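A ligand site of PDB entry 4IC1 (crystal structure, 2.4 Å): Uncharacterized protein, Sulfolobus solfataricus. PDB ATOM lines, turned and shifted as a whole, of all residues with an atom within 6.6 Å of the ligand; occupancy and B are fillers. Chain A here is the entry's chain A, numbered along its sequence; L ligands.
The side-chain sulfur (SG) of Cys 195 lies close to the backbone NH (N) of Phe 197, at 3.5 Å. NH2 of Arg 39 lies within salt-bridge range of OE2 of Glu 191, at 3.3 Å. The backbone NH (N) of Ala 203 sits close to the side-chain sulfur (SG) of Cys 201, at 3.3 Å. NE of Arg 38 lies close to SG of Cys 201, at 3.3 Å. The backbone NH (N) of Arg 39 sits close to the side-chain sulfur (SG) of Cys 36, at 3.6 Å. NH1 of Arg 38 lies within hydrogen-bond range of OH of Tyr 42 (3.0 Å). The backbone NH of Arg 38 lies close to the side-chain sulfur of Cys 36, at 3.3 Å. The side-chain carboxylate (OE2) of Glu 191 sits at hydrogen-bond distance from the backbone NH (N) of Cys 36 (3.0 Å).
Residues that only touch the ligand: Arg 39 (3.9 Å), Ser 198 (3.9 Å) and Arg 38 (3.98 Å). Of the 24 residues printed, 7 come within 4 Å of the ligand.
An iron atom (FE4) of the ligand is bound by the side-chain sulfur of Cys 195, at 2.1 Å. FE2 of the ligand is bound by SG of Cys 36, 2.3 Å away. An iron atom (FE3) of the ligand is bound by the side-chain sulfur of Cys 192, 2.1 Å away. The side-chain sulfur (SG) of Cys 201 binds an iron atom (FE1) of the ligand.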
ATOM      1  N   CYS A  36     -26.556  -4.387  28.178  1.00  0.00           N
ATOM      2  CA  CYS A  36     -25.622  -3.351  28.644  1.00  0.00           C
ATOM      3  C   CYS A  36     -25.641  -2.163  27.725  1.00  0.00           C
ATOM      4  O   CYS A  36     -25.476  -2.296  26.513  1.00  0.00           O
ATOM      5  CB  CYS A  36     -24.202  -3.906  28.793  1.00  0.00           C
ATOM      6  SG  CYS A  36     -23.063  -2.616  29.121  1.00  0.00           S
ATOM      7  N   PRO A  37     -25.895  -0.978  28.276  1.00  0.00           N
ATOM      8  CA  PRO A  37     -25.916   0.171  27.401  1.00  0.00           C
ATOM      9  C   PRO A  37     -24.615   0.383  26.687  1.00  0.00           C
ATOM     10  O   PRO A  37     -24.639   0.759  25.527  1.00  0.00           O
ATOM     11  CB  PRO A  37     -26.189   1.351  28.343  1.00  0.00           C
ATOM     12  CG  PRO A  37     -26.763   0.788  29.495  1.00  0.00           C
ATOM     13  CD  PRO A  37     -26.194  -0.609  29.654  1.00  0.00           C
ATOM     14  N   ARG A  38     -23.481   0.121  27.303  1.00  0.00           N
ATOM     15  CA  ARG A  38     -22.214   0.317  26.582  1.00  0.00           C
ATOM     16  C   ARG A  38     -22.078  -0.672  25.462  1.00  0.00           C
ATOM     17  O   ARG A  38     -21.592  -0.336  24.417  1.00  0.00           O
ATOM     18  CB  ARG A  38     -21.002   0.215  27.489  1.00  0.00           C
ATOM     19  CG  ARG A  38     -20.794   1.332  28.517  1.00  0.00           C
ATOM     20  CD  ARG A  38     -19.418   1.107  29.190  1.00  0.00           C
ATOM     21  NE  ARG A  38     -18.318   1.400  28.267  1.00  0.00           N
ATOM     22  CZ  ARG A  38     -17.905   2.626  27.981  1.00  0.00           C
ATOM     23  NH1 ARG A  38     -16.939   2.794  27.083  1.00  0.00           N
ATOM     24  NH2 ARG A  38     -18.456   3.660  28.609  1.00  0.00           N
ATOM     25  N   ARG A  39     -22.555  -1.892  25.648  1.00  0.00           N
ATOM     26  CA  ARG A  39     -22.376  -2.881  24.664  1.00  0.00           C
ATOM     27  C   ARG A  39     -23.185  -2.489  23.446  1.00  0.00           C
ATOM     28  O   ARG A  39     -22.762  -2.655  22.326  1.00  0.00           O
ATOM     29  CB  ARG A  39     -22.886  -4.123  25.231  1.00  0.00           C
ATOM     30  CG  ARG A  39     -22.700  -5.360  24.412  1.00  0.00           C
ATOM     31  CD  ARG A  39     -23.248  -6.479  25.308  1.00  0.00           C
ATOM     32  NE  ARG A  39     -22.778  -7.806  24.960  1.00  0.00           N
ATOM     33  CZ  ARG A  39     -22.941  -8.867  25.739  1.00  0.00           C
ATOM     34  NH1 ARG A  39     -22.487 -10.061  25.339  1.00  0.00           N
ATOM     35  NH2 ARG A  39     -23.583  -8.750  26.899  1.00  0.00           N
ATOM     36  N   VAL A  40     -24.375  -1.933  23.696  1.00  0.00           N
ATOM     37  CA  VAL A  40     -25.238  -1.485  22.629  1.00  0.00           C
ATOM     38  C   VAL A  40     -24.532  -0.423  21.840  1.00  0.00           C
ATOM     39  O   VAL A  40     -24.563  -0.472  20.609  1.00  0.00           O
ATOM     40  CB  VAL A  40     -26.622  -1.028  23.163  1.00  0.00           C
ATOM     41  CG1 VAL A  40     -27.485  -0.430  22.066  1.00  0.00           C
ATOM     42  CG2 VAL A  40     -27.339  -2.240  23.889  1.00  0.00           C
ATOM     43  N   TYR A  42     -21.204   0.169  21.689  1.00  0.00           N
ATOM     44  CA  TYR A  42     -20.108  -0.505  20.942  1.00  0.00           C
ATOM     45  C   TYR A  42     -20.545  -1.125  19.636  1.00  0.00           C
ATOM     46  O   TYR A  42     -19.809  -1.073  18.660  1.00  0.00           O
ATOM     47  CB  TYR A  42     -19.357  -1.567  21.753  1.00  0.00           C
ATOM     48  CG  TYR A  42     -18.383  -1.016  22.784  1.00  0.00           C
ATOM     49  CD1 TYR A  42     -17.277  -0.340  22.407  1.00  0.00           C
ATOM     50  CD2 TYR A  42     -18.585  -1.201  24.122  1.00  0.00           C
ATOM     51  CE1 TYR A  42     -16.394   0.149  23.330  1.00  0.00           C
ATOM     52  CE2 TYR A  42     -17.726  -0.715  25.072  1.00  0.00           C
ATOM     53  CZ  TYR A  42     -16.637  -0.032  24.668  1.00  0.00           C
ATOM     54  OH  TYR A  42     -15.777   0.486  25.613  1.00  0.00           O
ATOM     55  N   SER A 185     -23.881   0.314  33.525  1.00  0.00           N
ATOM     56  CA  SER A 185     -23.208  -0.747  32.768  1.00  0.00           C
ATOM     57  C   SER A 185     -22.300  -1.621  33.637  1.00  0.00           C
ATOM     58  O   SER A 185     -21.478  -1.124  34.345  1.00  0.00           O
ATOM     59  CB  SER A 185     -22.387  -0.121  31.647  1.00  0.00           C
ATOM     60  OG  SER A 185     -23.220   0.669  30.806  1.00  0.00           O
ATOM     61  N   PRO A 186     -22.399  -2.931  33.528  1.00  0.00           N
ATOM     62  CA  PRO A 186     -23.298  -3.617  32.669  1.00  0.00           C
ATOM     63  C   PRO A 186     -24.685  -3.647  33.286  1.00  0.00           C
ATOM     64  O   PRO A 186     -24.831  -3.515  34.493  1.00  0.00           O
ATOM     65  CB  PRO A 186     -22.717  -5.015  32.626  1.00  0.00           C
ATOM     66  CG  PRO A 186     -22.077  -5.199  33.908  1.00  0.00           C
ATOM     67  CD  PRO A 186     -21.520  -3.855  34.244  1.00  0.00           C
ATOM     68  N   ARG A 187     -25.696  -3.889  32.468  1.00  0.00           N
ATOM     69  CA  ARG A 187     -26.996  -4.075  33.050  1.00  0.00           C
ATOM     70  C   ARG A 187     -26.992  -5.265  34.036  1.00  0.00           C
ATOM     71  O   ARG A 187     -27.577  -5.120  35.084  1.00  0.00           O
ATOM     72  CB  ARG A 187     -28.031  -4.268  31.997  1.00  0.00           C
ATOM     73  CG  ARG A 187     -29.419  -3.958  32.499  1.00  0.00           C
ATOM     74  CD  ARG A 187     -30.465  -3.970  31.362  1.00  0.00           C
ATOM     75  NE  ARG A 187     -30.286  -2.950  30.318  1.00  0.00           N
ATOM     76  CZ  ARG A 187     -30.746  -1.700  30.385  1.00  0.00           C
ATOM     77  NH1 ARG A 187     -31.355  -1.268  31.492  1.00  0.00           N
ATOM     78  NH2 ARG A 187     -30.574  -0.855  29.346  1.00  0.00           N
ATOM     79  N   PHE A 188     -26.294  -6.378  33.734  1.00  0.00           N
ATOM     80  CA  PHE A 188     -26.320  -7.616  34.516  1.00  0.00           C
ATOM     81  C   PHE A 188     -24.888  -8.066  34.697  1.00  0.00           C
ATOM     82  O   PHE A 188     -24.130  -8.113  33.746  1.00  0.00           O
ATOM     83  CB  PHE A 188     -27.123  -8.768  33.848  1.00  0.00           C
ATOM     84  CG  PHE A 188     -28.568  -8.426  33.594  1.00  0.00           C
ATOM     85  CD1 PHE A 188     -29.458  -8.233  34.650  1.00  0.00           C
ATOM     86  CD2 PHE A 188     -29.037  -8.221  32.330  1.00  0.00           C
ATOM     87  CE1 PHE A 188     -30.798  -7.817  34.388  1.00  0.00           C
ATOM     88  CE2 PHE A 188     -30.332  -7.792  32.083  1.00  0.00           C
ATOM     89  CZ  PHE A 188     -31.206  -7.609  33.079  1.00  0.00           C
ATOM     90  N   GLU A 191     -22.741 -10.202  32.147  1.00  0.00           N
ATOM     91  CA  GLU A 191     -22.555  -9.808  30.743  1.00  0.00           C
ATOM     92  C   GLU A 191     -21.103  -9.726  30.301  1.00  0.00           C
ATOM     93  O   GLU A 191     -20.745 -10.160  29.221  1.00  0.00           O
ATOM     94  CB  GLU A 191     -23.248  -8.469  30.421  1.00  0.00           C
ATOM     95  CG  GLU A 191     -24.723  -8.552  30.469  1.00  0.00           C
ATOM     96  CD  GLU A 191     -25.379  -7.291  30.058  1.00  0.00           C
ATOM     97  OE1 GLU A 191     -25.478  -6.408  30.969  1.00  0.00           O
ATOM     98  OE2 GLU A 191     -25.751  -7.196  28.832  1.00  0.00           O
ATOM     99  N   CYS A 192     -20.273  -9.114  31.148  1.00  0.00           N
ATOM    100  CA  CYS A 192     -18.867  -8.834  30.814  1.00  0.00           C
ATOM    101  C   CYS A 192     -18.122 -10.092  30.396  1.00  0.00           C
ATOM    102  O   CYS A 192     -17.363 -10.098  29.444  1.00  0.00           O
ATOM    103  CB  CYS A 192     -18.201  -8.138  31.990  1.00  0.00           C
ATOM    104  SG  CYS A 192     -18.986  -6.515  32.340  1.00  0.00           S
ATOM    105  N   LYS A 193     -18.436 -11.167  31.060  1.00  0.00           N
ATOM    106  CA  LYS A 193     -17.707 -12.376  30.867  1.00  0.00           C
ATOM    107  C   LYS A 193     -17.725 -12.826  29.428  1.00  0.00           C
ATOM    108  O   LYS A 193     -16.819 -13.483  29.001  1.00  0.00           O
ATOM    109  CB  LYS A 193     -18.278 -13.471  31.753  1.00  0.00           C
ATOM    110  CG  LYS A 193     -17.434 -14.749  31.749  1.00  0.00           C
ATOM    111  CD  LYS A 193     -17.971 -15.871  32.653  1.00  0.00           C
ATOM    112  CE  LYS A 193     -17.626 -17.341  32.155  1.00  0.00           C
ATOM    113  NZ  LYS A 193     -18.513 -18.415  32.835  1.00  0.00           N
ATOM    114  N   TYR A 194     -18.766 -12.493  28.670  1.00  0.00           N
ATOM    115  CA  TYR A 194     -18.901 -12.998  27.309  1.00  0.00           C
ATOM    116  C   TYR A 194     -18.885 -11.899  26.257  1.00  0.00           C
ATOM    117  O   TYR A 194     -19.108 -12.198  25.088  1.00  0.00           O
ATOM    118  CB  TYR A 194     -20.245 -13.725  27.132  1.00  0.00           C
ATOM    119  CG  TYR A 194     -20.636 -14.695  28.183  1.00  0.00           C
ATOM    120  CD1 TYR A 194     -20.173 -16.023  28.150  1.00  0.00           C
ATOM    121  CD2 TYR A 194     -21.487 -14.300  29.232  1.00  0.00           C
ATOM    122  CE1 TYR A 194     -20.537 -16.942  29.133  1.00  0.00           C
ATOM    123  CE2 TYR A 194     -21.859 -15.220  30.227  1.00  0.00           C
ATOM    124  CZ  TYR A 194     -21.390 -16.523  30.167  1.00  0.00           C
ATOM    125  OH  TYR A 194     -21.801 -17.398  31.160  1.00  0.00           O
ATOM    126  N   CYS A 195     -18.711 -10.661  26.690  1.00  0.00           N
ATOM    127  CA  CYS A 195     -18.766  -9.514  25.844  1.00  0.00           C
ATOM    128  C   CYS A 195     -17.451  -9.409  25.040  1.00  0.00           C
ATOM    129  O   CYS A 195     -16.369  -9.279  25.618  1.00  0.00           O
ATOM    130  CB  CYS A 195     -18.930  -8.288  26.761  1.00  0.00           C
ATOM    131  SG  CYS A 195     -19.011  -6.801  25.912  1.00  0.00           S
ATOM    132  N   ILE A 196     -17.544  -9.401  23.709  1.00  0.00           N
ATOM    133  CA  ILE A 196     -16.385  -9.143  22.828  1.00  0.00           C
ATOM    134  C   ILE A 196     -15.731  -7.722  22.992  1.00  0.00           C
ATOM    135  O   ILE A 196     -14.590  -7.551  22.610  1.00  0.00           O
ATOM    136  CB  ILE A 196     -16.737  -9.383  21.324  1.00  0.00           C
ATOM    137  CG1 ILE A 196     -17.763  -8.381  20.794  1.00  0.00           C
ATOM    138  CG2 ILE A 196     -17.322 -10.777  21.098  1.00  0.00           C
ATOM    139  CD1 ILE A 196     -18.050  -8.548  19.249  1.00  0.00           C
ATOM    140  N   PHE A 197     -16.433  -6.742  23.601  1.00  0.00           N
ATOM    141  CA  PHE A 197     -15.872  -5.384  23.866  1.00  0.00           C
ATOM    142  C   PHE A 197     -15.189  -5.259  25.227  1.00  0.00           C
ATOM    143  O   PHE A 197     -14.627  -4.220  25.601  1.00  0.00           O
ATOM    144  CB  PHE A 197     -16.968  -4.327  23.764  1.00  0.00           C
ATOM    145  CG  PHE A 197     -17.693  -4.400  22.476  1.00  0.00           C
ATOM    146  CD1 PHE A 197     -17.072  -4.032  21.302  1.00  0.00           C
ATOM    147  CD2 PHE A 197     -18.945  -4.981  22.394  1.00  0.00           C
ATOM    148  CE1 PHE A 197     -17.686  -4.196  20.106  1.00  0.00           C
ATOM    149  CE2 PHE A 197     -19.552  -5.112  21.182  1.00  0.00           C
ATOM    150  CZ  PHE A 197     -18.928  -4.712  20.057  1.00  0.00           C
ATOM    151  N   SER A 198     -15.197  -6.336  26.009  1.00  0.00           N
ATOM    152  CA  SER A 198     -14.532  -6.279  27.307  1.00  0.00           C
ATOM    153  C   SER A 198     -13.092  -5.891  27.135  1.00  0.00           C
ATOM    154  O   SER A 198     -12.546  -5.242  28.035  1.00  0.00           O
ATOM    155  CB  SER A 198     -14.587  -7.616  28.032  1.00  0.00           C
ATOM    156  OG  SER A 198     -14.038  -8.675  27.273  1.00  0.00           O
ATOM    157  N   VAL A 199     -12.498  -6.244  25.997  1.00  0.00           N
ATOM    158  CA  VAL A 199     -11.043  -6.026  25.795  1.00  0.00           C
ATOM    159  C   VAL A 199     -10.674  -4.561  25.667  1.00  0.00           C
ATOM    160  O   VAL A 199      -9.507  -4.179  25.861  1.00  0.00           O
ATOM    161  CB  VAL A 199     -10.520  -6.803  24.611  1.00  0.00           C
ATOM    162  CG1 VAL A 199     -10.685  -8.314  24.872  1.00  0.00           C
ATOM    163  CG2 VAL A 199     -11.190  -6.358  23.363  1.00  0.00           C
ATOM    164  N   CYS A 201     -13.126  -2.110  27.139  1.00  0.00           N
ATOM    165  CA  CYS A 201     -14.114  -1.385  27.935  1.00  0.00           C
ATOM    166  C   CYS A 201     -13.676  -1.095  29.358  1.00  0.00           C
ATOM    167  O   CYS A 201     -13.316  -1.993  30.095  1.00  0.00           O
ATOM    168  CB  CYS A 201     -15.412  -2.144  28.003  1.00  0.00           C
ATOM    169  SG  CYS A 201     -16.762  -1.371  29.040  1.00  0.00           S
ATOM    170  N   PRO A 202     -13.774   0.153  29.771  1.00  0.00           N
ATOM    171  CA  PRO A 202     -13.358   0.538  31.083  1.00  0.00           C
ATOM    172  C   PRO A 202     -14.256   0.099  32.232  1.00  0.00           C
ATOM    173  O   PRO A 202     -13.776   0.081  33.377  1.00  0.00           O
ATOM    174  CB  PRO A 202     -13.291   2.082  31.010  1.00  0.00           C
ATOM    175  CG  PRO A 202     -14.119   2.457  29.887  1.00  0.00           C
ATOM    176  CD  PRO A 202     -14.280   1.280  28.982  1.00  0.00           C
ATOM    177  N   ALA A 203     -15.507  -0.255  31.937  1.00  0.00           N
ATOM    178  CA  ALA A 203     -16.472  -0.634  32.967  1.00  0.00           C
ATOM    179  C   ALA A 203     -16.553  -2.134  33.190  1.00  0.00           C
ATOM    180  O   ALA A 203     -17.314  -2.583  34.010  1.00  0.00           O
ATOM    181  CB  ALA A 203     -17.800  -0.118  32.610  1.00  0.00           C
ATOM    182  N   LYS A 204     -15.770  -2.912  32.449  1.00  0.00           N
ATOM    183  CA  LYS A 204     -15.768  -4.348  32.615  1.00  0.00           C
ATOM    184  C   LYS A 204     -15.603  -4.691  34.054  1.00  0.00           C
ATOM    185  O   LYS A 204     -14.706  -4.153  34.723  1.00  0.00           O
ATOM    186  CB  LYS A 204     -14.595  -4.949  31.876  1.00  0.00           C
ATOM    187  CG  LYS A 204     -14.369  -6.435  32.084  1.00  0.00           C
ATOM    188  CD  LYS A 204     -12.950  -6.768  31.632  1.00  0.00           C
ATOM    189  CE  LYS A 204     -12.620  -8.236  31.799  1.00  0.00           C
ATOM    190  NZ  LYS A 204     -11.239  -8.626  31.238  1.00  0.00           N
ATOM    191  N   LEU A 205     -16.433  -5.636  34.519  1.00  0.00           N
ATOM    192  CA  LEU A 205     -16.376  -6.117  35.880  1.00  0.00           C
ATOM    193  C   LEU A 205     -15.217  -7.054  35.963  1.00  0.00           C
ATOM    194  O   LEU A 205     -15.079  -7.904  35.124  1.00  0.00           O
ATOM    195  CB  LEU A 205     -17.669  -6.846  36.257  1.00  0.00           C
ATOM    196  CG  LEU A 205     -18.952  -5.975  36.356  1.00  0.00           C
ATOM    197  CD1 LEU A 205     -20.100  -6.720  37.001  1.00  0.00           C
ATOM    198  CD2 LEU A 205     -18.717  -4.666  37.074  1.00  0.00           C
HETATM  199 FE1  LIG L   1     -18.150  -3.127  29.013  1.00  0.00          FE
HETATM  200 FE2  LIG L   1     -21.048  -3.660  28.973  1.00  0.00          FE
HETATM  201 FE3  LIG L   1     -19.261  -5.391  30.584  1.00  0.00          FE
HETATM  202 FE4  LIG L   1     -19.173  -5.479  27.584  1.00  0.00          FE
HETATM  203  S1  LIG L   1     -20.619  -5.665  29.061  1.00  0.00           S
HETATM  204  S2  LIG L   1     -17.838  -5.128  29.087  1.00  0.00           S
HETATM  205  S3  LIG L   1     -19.556  -3.493  27.565  1.00  0.00           S
HETATM  206  S4  LIG L   1     -19.639  -3.405  30.459  1.00  0.00           S
